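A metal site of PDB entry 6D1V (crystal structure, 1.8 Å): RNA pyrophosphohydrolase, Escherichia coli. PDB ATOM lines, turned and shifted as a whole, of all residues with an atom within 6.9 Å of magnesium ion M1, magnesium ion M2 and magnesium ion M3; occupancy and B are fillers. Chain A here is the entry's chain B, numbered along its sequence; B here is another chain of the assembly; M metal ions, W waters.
Magnesium ion M3 is bound by O3G of APC 1 of chain B (1.9 Å), the backbone carbonyl oxygen (O) of Gln 38 (2.0 Å), the side-chain carboxylate (OE2) of Glu 58 (2.0 Å), O2B of APC 1 of chain B (2.0 Å), the side-chain carboxylate (OE1) of Glu 121 (2.0 Å) and water W5 (2.1 Å).
O1B of APC 1 of chain B lies close to N of Gly 40.
O1A of APC 1 of chain B lies within salt-bridge range of the guanidinium group of Arg 9.
O1G of APC 1 of chain B sits at hydrogen-bond distance from the side-chain amide nitrogen (ND2) of Asn 11 (3.2 Å).
The side-chain carboxylate of Glu 54 lies close to the guanidinium group of Arg 53 (3.4 Å).
The side-chain carboxylate of Glu 57 is in salt-bridge range of the guanidinium group of Arg 53, at 3.98 Å.
O of Gly 40 lies within hydrogen-bond range of NH1 of Arg 53 (2.9 Å).
The backbone carbonyl oxygen (O) of Gly 39 sits close to the side-chain amide nitrogen (ND2) of Asn 11 (3.4 Å).
The backbone NH (N) of Val 12 lies within hydrogen-bond range of the backbone carbonyl oxygen (O) of Gly 39, at 2.9 Å.
OE2 of Glu 54 is bound to magnesium ion M2, 2.0 Å away.
Magnesium ion M2 is bound by O1B of APC 1 of chain B.
Water W2 is bound to magnesium ion M2 (2.1 Å).
Magnesium ion M2 is bound by water W4 (2.1 Å).
Water W3 is bound to magnesium ion M2.
Water W1 is bound to magnesium ion M2 (2.3 Å).
Magnesium ion M2 has six donor atoms within binding distance.
CA of Gly 39 touches magnesium ion M3, 3.9 Å away.
The nearest printed residue that does not touch magnesium ion M3 is Glu 57 (4.8 Å).
Gly 40 touches magnesium ion M2.
Four residues have an atom within 4 Å of magnesium ion M2: Gly 40, Glu 54, Glu 57 and APC 1 of chain B.
Along chain A the residues within 4 Å of magnesium ion M2 span positions 40 to 57.
The nearest printed residue that does not touch magnesium ion M1 is Gln 38 (4.03 Å).
Magnesium ion M1 is bound by the side-chain carboxylate of Glu 54 (2.0 Å), the side-chain carboxylate of Glu 121 (2.0 Å), O2B of APC 1 of chain B (2.1 Å), the side-chain carboxylate of Glu 57 (2.1 Å), the side-chain carboxylate of Glu 58 (2.2 Å) and water W2 (2.2 Å).
Water W4 bridges O of Gly 40 and NH1 of Arg 53.
Water W1 bridges NH2 of Arg 53 (2.7 Å) and OE2 of Glu 57 (2.9 Å).
Water W5 bridges the side-chain carboxylate (OE1) of Glu 58 (2.8 Å) and the backbone NH (N) of Gln 38 (3.4 Å).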
ATOM      1  N   ARG A   9       9.199 -21.957 -26.212  1.00  0.00           N
ATOM      2  CA  ARG A   9      10.275 -21.526 -25.331  1.00  0.00           C
ATOM      3  C   ARG A   9      11.625 -21.889 -25.936  1.00  0.00           C
ATOM      4  O   ARG A   9      11.840 -23.057 -26.305  1.00  0.00           O
ATOM      5  CB  ARG A   9      10.118 -22.171 -23.950  1.00  0.00           C
ATOM      6  CG  ARG A   9      11.034 -21.593 -22.885  1.00  0.00           C
ATOM      7  CD  ARG A   9      10.776 -22.248 -21.539  1.00  0.00           C
ATOM      8  NE  ARG A   9      11.304 -23.609 -21.524  1.00  0.00           N
ATOM      9  CZ  ARG A   9      11.805 -24.213 -20.459  1.00  0.00           C
ATOM     10  NH1 ARG A   9      11.861 -23.588 -19.291  1.00  0.00           N
ATOM     11  NH2 ARG A   9      12.261 -25.465 -20.578  1.00  0.00           N
ATOM     12  N   ASN A  11      15.364 -23.138 -25.994  1.00  0.00           N
ATOM     13  CA  ASN A  11      15.725 -24.307 -25.200  1.00  0.00           C
ATOM     14  C   ASN A  11      17.014 -24.894 -25.772  1.00  0.00           C
ATOM     15  O   ASN A  11      17.280 -24.736 -26.966  1.00  0.00           O
ATOM     16  CB  ASN A  11      14.545 -25.307 -25.217  1.00  0.00           C
ATOM     17  CG  ASN A  11      14.826 -26.592 -24.455  1.00  0.00           C
ATOM     18  OD1 ASN A  11      15.651 -27.416 -24.884  1.00  0.00           O
ATOM     19  ND2 ASN A  11      14.096 -26.805 -23.359  1.00  0.00           N
ATOM     20  N   VAL A  12      17.828 -25.529 -24.919  1.00  0.00           N
ATOM     21  CA  VAL A  12      19.035 -26.224 -25.371  1.00  0.00           C
ATOM     22  C   VAL A  12      18.951 -27.690 -24.965  1.00  0.00           C
ATOM     23  O   VAL A  12      18.533 -28.018 -23.849  1.00  0.00           O
ATOM     24  CB  VAL A  12      20.342 -25.608 -24.829  1.00  0.00           C
ATOM     25  CG1 VAL A  12      20.527 -24.193 -25.377  1.00  0.00           C
ATOM     26  CG2 VAL A  12      20.361 -25.631 -23.318  1.00  0.00           C
ATOM     27  N   GLN A  35      15.399 -39.628 -21.243  1.00  0.00           N
ATOM     28  CA  GLN A  35      15.550 -38.615 -22.286  1.00  0.00           C
ATOM     29  C   GLN A  35      16.973 -38.074 -22.206  1.00  0.00           C
ATOM     30  O   GLN A  35      17.716 -38.374 -21.275  1.00  0.00           O
ATOM     31  CB  GLN A  35      14.553 -37.478 -22.088  1.00  0.00           C
ATOM     32  CG  GLN A  35      14.924 -36.695 -20.795  1.00  0.00           C
ATOM     33  CD  GLN A  35      14.018 -35.496 -20.538  1.00  0.00           C
ATOM     34  OE1 GLN A  35      12.992 -35.600 -19.887  1.00  0.00           O
ATOM     35  NE2 GLN A  35      14.423 -34.331 -21.017  1.00  0.00           N
ATOM     36  N   PHE A  36      17.310 -37.235 -23.192  1.00  0.00           N
ATOM     37  CA  PHE A  36      18.534 -36.455 -23.085  1.00  0.00           C
ATOM     38  C   PHE A  36      18.274 -35.230 -22.210  1.00  0.00           C
ATOM     39  O   PHE A  36      17.142 -34.726 -22.175  1.00  0.00           O
ATOM     40  CB  PHE A  36      18.963 -35.968 -24.459  1.00  0.00           C
ATOM     41  CG  PHE A  36      19.516 -37.029 -25.386  1.00  0.00           C
ATOM     42  CD1 PHE A  36      20.426 -37.976 -24.944  1.00  0.00           C
ATOM     43  CD2 PHE A  36      19.186 -37.002 -26.743  1.00  0.00           C
ATOM     44  CE1 PHE A  36      20.969 -38.918 -25.813  1.00  0.00           C
ATOM     45  CE2 PHE A  36      19.748 -37.933 -27.640  1.00  0.00           C
ATOM     46  CZ  PHE A  36      20.619 -38.885 -27.184  1.00  0.00           C
ATOM     47  N   PRO A  37      19.295 -34.705 -21.531  1.00  0.00           N
ATOM     48  CA  PRO A  37      19.132 -33.426 -20.818  1.00  0.00           C
ATOM     49  C   PRO A  37      18.755 -32.316 -21.781  1.00  0.00           C
ATOM     50  O   PRO A  37      19.295 -32.223 -22.895  1.00  0.00           O
ATOM     51  CB  PRO A  37      20.516 -33.159 -20.208  1.00  0.00           C
ATOM     52  CG  PRO A  37      21.219 -34.526 -20.165  1.00  0.00           C
ATOM     53  CD  PRO A  37      20.648 -35.271 -21.372  1.00  0.00           C
ATOM     54  N   GLN A  38      17.862 -31.439 -21.328  1.00  0.00           N
ATOM     55  CA  GLN A  38      17.535 -30.196 -22.022  1.00  0.00           C
ATOM     56  C   GLN A  38      17.024 -29.182 -21.002  1.00  0.00           C
ATOM     57  O   GLN A  38      16.562 -29.549 -19.920  1.00  0.00           O
ATOM     58  CB  GLN A  38      16.467 -30.383 -23.098  1.00  0.00           C
ATOM     59  CG  GLN A  38      15.177 -30.951 -22.564  1.00  0.00           C
ATOM     60  CD  GLN A  38      14.129 -31.074 -23.634  1.00  0.00           C
ATOM     61  OE1 GLN A  38      14.302 -31.810 -24.612  1.00  0.00           O
ATOM     62  NE2 GLN A  38      13.026 -30.352 -23.473  1.00  0.00           N
ATOM     63  N   GLY A  39      17.042 -27.906 -21.390  1.00  0.00           N
ATOM     64  CA  GLY A  39      16.658 -26.858 -20.446  1.00  0.00           C
ATOM     65  C   GLY A  39      16.379 -25.537 -21.130  1.00  0.00           C
ATOM     66  O   GLY A  39      16.874 -25.273 -22.237  1.00  0.00           O
ATOM     67  N   GLY A  40      15.567 -24.725 -20.464  1.00  0.00           N
ATOM     68  CA  GLY A  40      15.170 -23.434 -21.031  1.00  0.00           C
ATOM     69  C   GLY A  40      16.308 -22.424 -20.981  1.00  0.00           C
ATOM     70  O   GLY A  40      17.087 -22.366 -20.019  1.00  0.00           O
ATOM     71  N   ILE A  41      16.415 -21.634 -22.049  1.00  0.00           N
ATOM     72  CA  ILE A  41      17.371 -20.534 -22.119  1.00  0.00           C
ATOM     73  C   ILE A  41      16.813 -19.345 -21.348  1.00  0.00           C
ATOM     74  O   ILE A  41      15.639 -18.987 -21.498  1.00  0.00           O
ATOM     75  CB  ILE A  41      17.663 -20.160 -23.574  1.00  0.00           C
ATOM     76  CG1 ILE A  41      18.390 -21.295 -24.283  1.00  0.00           C
ATOM     77  CG2 ILE A  41      18.483 -18.867 -23.644  1.00  0.00           C
ATOM     78  CD1 ILE A  41      18.721 -21.029 -25.752  1.00  0.00           C
ATOM     79  N   ASN A  42      17.643 -18.738 -20.504  1.00  0.00           N
ATOM     80  CA  ASN A  42      17.169 -17.682 -19.625  1.00  0.00           C
ATOM     81  C   ASN A  42      17.347 -16.310 -20.262  1.00  0.00           C
ATOM     82  O   ASN A  42      18.190 -16.136 -21.163  1.00  0.00           O
ATOM     83  CB  ASN A  42      17.904 -17.758 -18.291  1.00  0.00           C
ATOM     84  CG  ASN A  42      17.238 -18.718 -17.345  1.00  0.00           C
ATOM     85  OD1 ASN A  42      16.028 -18.909 -17.385  1.00  0.00           O
ATOM     86  ND2 ASN A  42      18.031 -19.360 -16.495  1.00  0.00           N
ATOM     87  N   ARG A  53      25.027 -24.130 -18.099  1.00  0.00           N
ATOM     88  CA  ARG A  53      24.246 -23.975 -16.875  1.00  0.00           C
ATOM     89  C   ARG A  53      23.372 -25.197 -16.597  1.00  0.00           C
ATOM     90  O   ARG A  53      23.380 -25.736 -15.495  1.00  0.00           O
ATOM     91  CB  ARG A  53      23.384 -22.716 -16.953  1.00  0.00           C
ATOM     92  CG  ARG A  53      22.542 -22.459 -15.708  1.00  0.00           C
ATOM     93  CD  ARG A  53      21.771 -21.162 -15.816  1.00  0.00           C
ATOM     94  NE  ARG A  53      20.773 -21.207 -16.885  1.00  0.00           N
ATOM     95  CZ  ARG A  53      19.567 -21.737 -16.749  1.00  0.00           C
ATOM     96  NH1 ARG A  53      18.718 -21.736 -17.768  1.00  0.00           N
ATOM     97  NH2 ARG A  53      19.193 -22.266 -15.586  1.00  0.00           N
ATOM     98  N   GLU A  54      22.618 -25.629 -17.610  1.00  0.00           N
ATOM     99  CA  GLU A  54      21.740 -26.785 -17.451  1.00  0.00           C
ATOM    100  C   GLU A  54      22.551 -28.078 -17.368  1.00  0.00           C
ATOM    101  O   GLU A  54      22.148 -29.016 -16.688  1.00  0.00           O
ATOM    102  CB  GLU A  54      20.734 -26.845 -18.602  1.00  0.00           C
ATOM    103  CG  GLU A  54      19.681 -25.726 -18.594  1.00  0.00           C
ATOM    104  CD  GLU A  54      18.480 -25.982 -17.691  1.00  0.00           C
ATOM    105  OE1 GLU A  54      18.270 -27.128 -17.224  1.00  0.00           O
ATOM    106  OE2 GLU A  54      17.742 -25.006 -17.447  1.00  0.00           O
ATOM    107  N   GLU A  57      23.590 -28.275 -13.827  1.00  0.00           N
ATOM    108  CA  GLU A  57      22.382 -28.433 -13.016  1.00  0.00           C
ATOM    109  C   GLU A  57      21.795 -29.850 -13.101  1.00  0.00           C
ATOM    110  O   GLU A  57      21.361 -30.423 -12.095  1.00  0.00           O
ATOM    111  CB  GLU A  57      21.344 -27.416 -13.464  1.00  0.00           C
ATOM    112  CG  GLU A  57      19.944 -27.635 -12.931  1.00  0.00           C
ATOM    113  CD  GLU A  57      18.882 -27.182 -13.928  1.00  0.00           C
ATOM    114  OE1 GLU A  57      18.211 -28.060 -14.547  1.00  0.00           O
ATOM    115  OE2 GLU A  57      18.735 -25.924 -14.086  1.00  0.00           O
ATOM    116  N   GLU A  58      21.786 -30.435 -14.295  1.00  0.00           N
ATOM    117  CA  GLU A  58      21.096 -31.710 -14.543  1.00  0.00           C
ATOM    118  C   GLU A  58      22.017 -32.914 -14.481  1.00  0.00           C
ATOM    119  O   GLU A  58      21.571 -33.992 -14.069  1.00  0.00           O
ATOM    120  CB  GLU A  58      20.412 -31.668 -15.927  1.00  0.00           C
ATOM    121  CG  GLU A  58      19.366 -30.551 -16.010  1.00  0.00           C
ATOM    122  CD  GLU A  58      18.362 -30.729 -17.128  1.00  0.00           C
ATOM    123  OE1 GLU A  58      18.504 -31.670 -17.948  1.00  0.00           O
ATOM    124  OE2 GLU A  58      17.416 -29.923 -17.195  1.00  0.00           O
ATOM    125  N   GLU A 121      16.167 -32.955 -11.975  1.00  0.00           N
ATOM    126  CA  GLU A 121      15.243 -33.416 -13.002  1.00  0.00           C
ATOM    127  C   GLU A 121      15.428 -34.897 -13.304  1.00  0.00           C
ATOM    128  O   GLU A 121      14.515 -35.523 -13.844  1.00  0.00           O
ATOM    129  CB  GLU A 121      15.411 -32.590 -14.278  1.00  0.00           C
ATOM    130  CG  GLU A 121      14.774 -31.228 -14.147  1.00  0.00           C
ATOM    131  CD  GLU A 121      15.140 -30.298 -15.280  1.00  0.00           C
ATOM    132  OE1 GLU A 121      14.844 -30.624 -16.475  1.00  0.00           O
ATOM    133  OE2 GLU A 121      15.727 -29.234 -14.956  1.00  0.00           O
ATOM    134  N   PHE A 122      16.562 -35.482 -12.934  1.00  0.00           N
ATOM    135  CA  PHE A 122      16.857 -36.876 -13.208  1.00  0.00           C
ATOM    136  C   PHE A 122      17.308 -37.597 -11.956  1.00  0.00           C
ATOM    137  O   PHE A 122      17.867 -36.993 -11.032  1.00  0.00           O
ATOM    138  CB  PHE A 122      17.951 -36.987 -14.244  1.00  0.00           C
ATOM    139  CG  PHE A 122      17.639 -36.359 -15.556  1.00  0.00           C
ATOM    140  CD1 PHE A 122      16.501 -36.737 -16.268  1.00  0.00           C
ATOM    141  CD2 PHE A 122      18.483 -35.403 -16.087  1.00  0.00           C
ATOM    142  CE1 PHE A 122      16.212 -36.151 -17.501  1.00  0.00           C
ATOM    143  CE2 PHE A 122      18.196 -34.818 -17.329  1.00  0.00           C
ATOM    144  CZ  PHE A 122      17.069 -35.194 -18.020  1.00  0.00           C
ATOM    145  PG  APC B   1      12.988 -28.944 -19.610  1.00  0.00           P
ATOM    146  O1G APC B   1      12.786 -28.698 -21.111  1.00  0.00           O
ATOM    147  O2G APC B   1      11.742 -29.301 -18.867  1.00  0.00           O
ATOM    148  O3G APC B   1      14.038 -29.930 -19.194  1.00  0.00           O
ATOM    149  PB  APC B   1      14.300 -27.053 -17.789  1.00  0.00           P
ATOM    150  O1B APC B   1      14.909 -25.585 -17.980  1.00  0.00           O
ATOM    151  O2B APC B   1      15.415 -28.002 -17.651  1.00  0.00           O
ATOM    152  O3B APC B   1      13.437 -27.443 -19.108  1.00  0.00           O
ATOM    153  PA  APC B   1      11.656 -26.315 -16.531  1.00  0.00           P
ATOM    154  O1A APC B   1      11.908 -24.743 -16.779  1.00  0.00           O
ATOM    155  O2A APC B   1      10.913 -26.540 -15.263  1.00  0.00           O
ATOM    156  C3A APC B   1      13.241 -27.214 -16.333  1.00  0.00           C
ATOM    157  O5' APC B   1      10.824 -26.982 -17.767  1.00  0.00           O
ATOM    158  C5' APC B   1       9.731 -27.860 -17.476  1.00  0.00           C
ATOM    159  C4' APC B   1       8.880 -28.212 -18.695  1.00  0.00           C
ATOM    160  O4' APC B   1       7.604 -27.756 -18.291  1.00  0.00           O
ATOM    161  C3' APC B   1       9.219 -27.429 -19.960  1.00  0.00           C
ATOM    162  O3' APC B   1       8.569 -28.044 -21.081  1.00  0.00           O
ATOM    163  C2' APC B   1       8.561 -26.083 -19.699  1.00  0.00           C
ATOM    164  O2' APC B   1       8.135 -25.392 -20.883  1.00  0.00           O
ATOM    165  C1' APC B   1       7.347 -26.476 -18.886  1.00  0.00           C
ATOM    166  N9  APC B   1       7.072 -25.443 -17.862  1.00  0.00           N
ATOM    167  C8  APC B   1       7.968 -24.709 -17.172  1.00  0.00           C
ATOM    168  N7  APC B   1       7.343 -23.839 -16.330  1.00  0.00           N
ATOM    169  C5  APC B   1       6.008 -24.026 -16.482  1.00  0.00           C
ATOM    170  C6  APC B   1       4.769 -23.461 -15.910  1.00  0.00           C
ATOM    171  N6  APC B   1       4.835 -22.481 -14.959  1.00  0.00           N
ATOM    172  N1  APC B   1       3.582 -23.948 -16.355  1.00  0.00           N
ATOM    173  C2  APC B   1       3.513 -24.912 -17.288  1.00  0.00           C
ATOM    174  N3  APC B   1       4.594 -25.475 -17.854  1.00  0.00           N
ATOM    175  C4  APC B   1       5.846 -25.076 -17.502  1.00  0.00           C
ATOM    176  P     G B   2       8.959 -29.519 -21.595  1.00  0.00           P
ATOM    177  OP1   G B   2      10.372 -29.817 -21.240  1.00  0.00           O
ATOM    178  OP2   G B   2       8.517 -29.631 -23.007  1.00  0.00           O
ATOM    179  O5'   G B   2       8.025 -30.462 -20.724  1.00  0.00           O
ATOM    180  C5'   G B   2       6.620 -30.343 -20.805  1.00  0.00           C
ATOM    181  C4'   G B   2       5.947 -31.607 -20.350  1.00  0.00           C
ATOM    182  O4'   G B   2       6.074 -32.605 -21.390  1.00  0.00           O
ATOM    183  C3'   G B   2       6.574 -32.261 -19.128  1.00  0.00           C
ATOM    184  O3'   G B   2       6.114 -31.719 -17.911  1.00  0.00           O
ATOM    185  C2'   G B   2       6.255 -33.740 -19.317  1.00  0.00           C
ATOM    186  O2'   G B   2       4.914 -34.024 -18.931  1.00  0.00           O
ATOM    187  C1'   G B   2       6.350 -33.874 -20.824  1.00  0.00           C
ATOM    188  N9    G B   2       7.666 -34.226 -21.253  1.00  0.00           N
ATOM    189  C8    G B   2       8.668 -33.388 -21.736  1.00  0.00           C
ATOM    190  N7    G B   2       9.744 -34.044 -22.091  1.00  0.00           N
ATOM    191  C5    G B   2       9.445 -35.398 -21.872  1.00  0.00           C
ATOM    192  C6    G B   2      10.210 -36.570 -22.093  1.00  0.00           C
ATOM    193  O6    G B   2      11.367 -36.664 -22.572  1.00  0.00           O
ATOM    194  N1    G B   2       9.500 -37.707 -21.726  1.00  0.00           N
ATOM    195  C2    G B   2       8.224 -37.738 -21.213  1.00  0.00           C
ATOM    196  N2    G B   2       7.735 -38.948 -20.927  1.00  0.00           N
ATOM    197  N3    G B   2       7.491 -36.652 -21.010  1.00  0.00           N
ATOM    198  C4    G B   2       8.163 -35.535 -21.360  1.00  0.00           C
HETATM  199 MG    MG M   1      16.857 -28.085 -16.173  1.00  0.00          MG
HETATM  200 MG    MG M   2      15.998 -24.620 -16.571  1.00  0.00          MG
HETATM  201 MG    MG M   3      15.678 -29.941 -18.201  1.00  0.00          MG
HETATM  202  O   HOH W   1      17.025 -23.642 -14.816  1.00  0.00           O
HETATM  203  O   HOH W   2      16.163 -26.219 -15.247  1.00  0.00           O
HETATM  204  O   HOH W   3      14.073 -23.929 -15.652  1.00  0.00           O
HETATM  205  O   HOH W   4      16.003 -22.954 -17.844  1.00  0.00           O
HETATM  206  O   HOH W   5      15.861 -32.032 -18.646  1.00  0.00           O
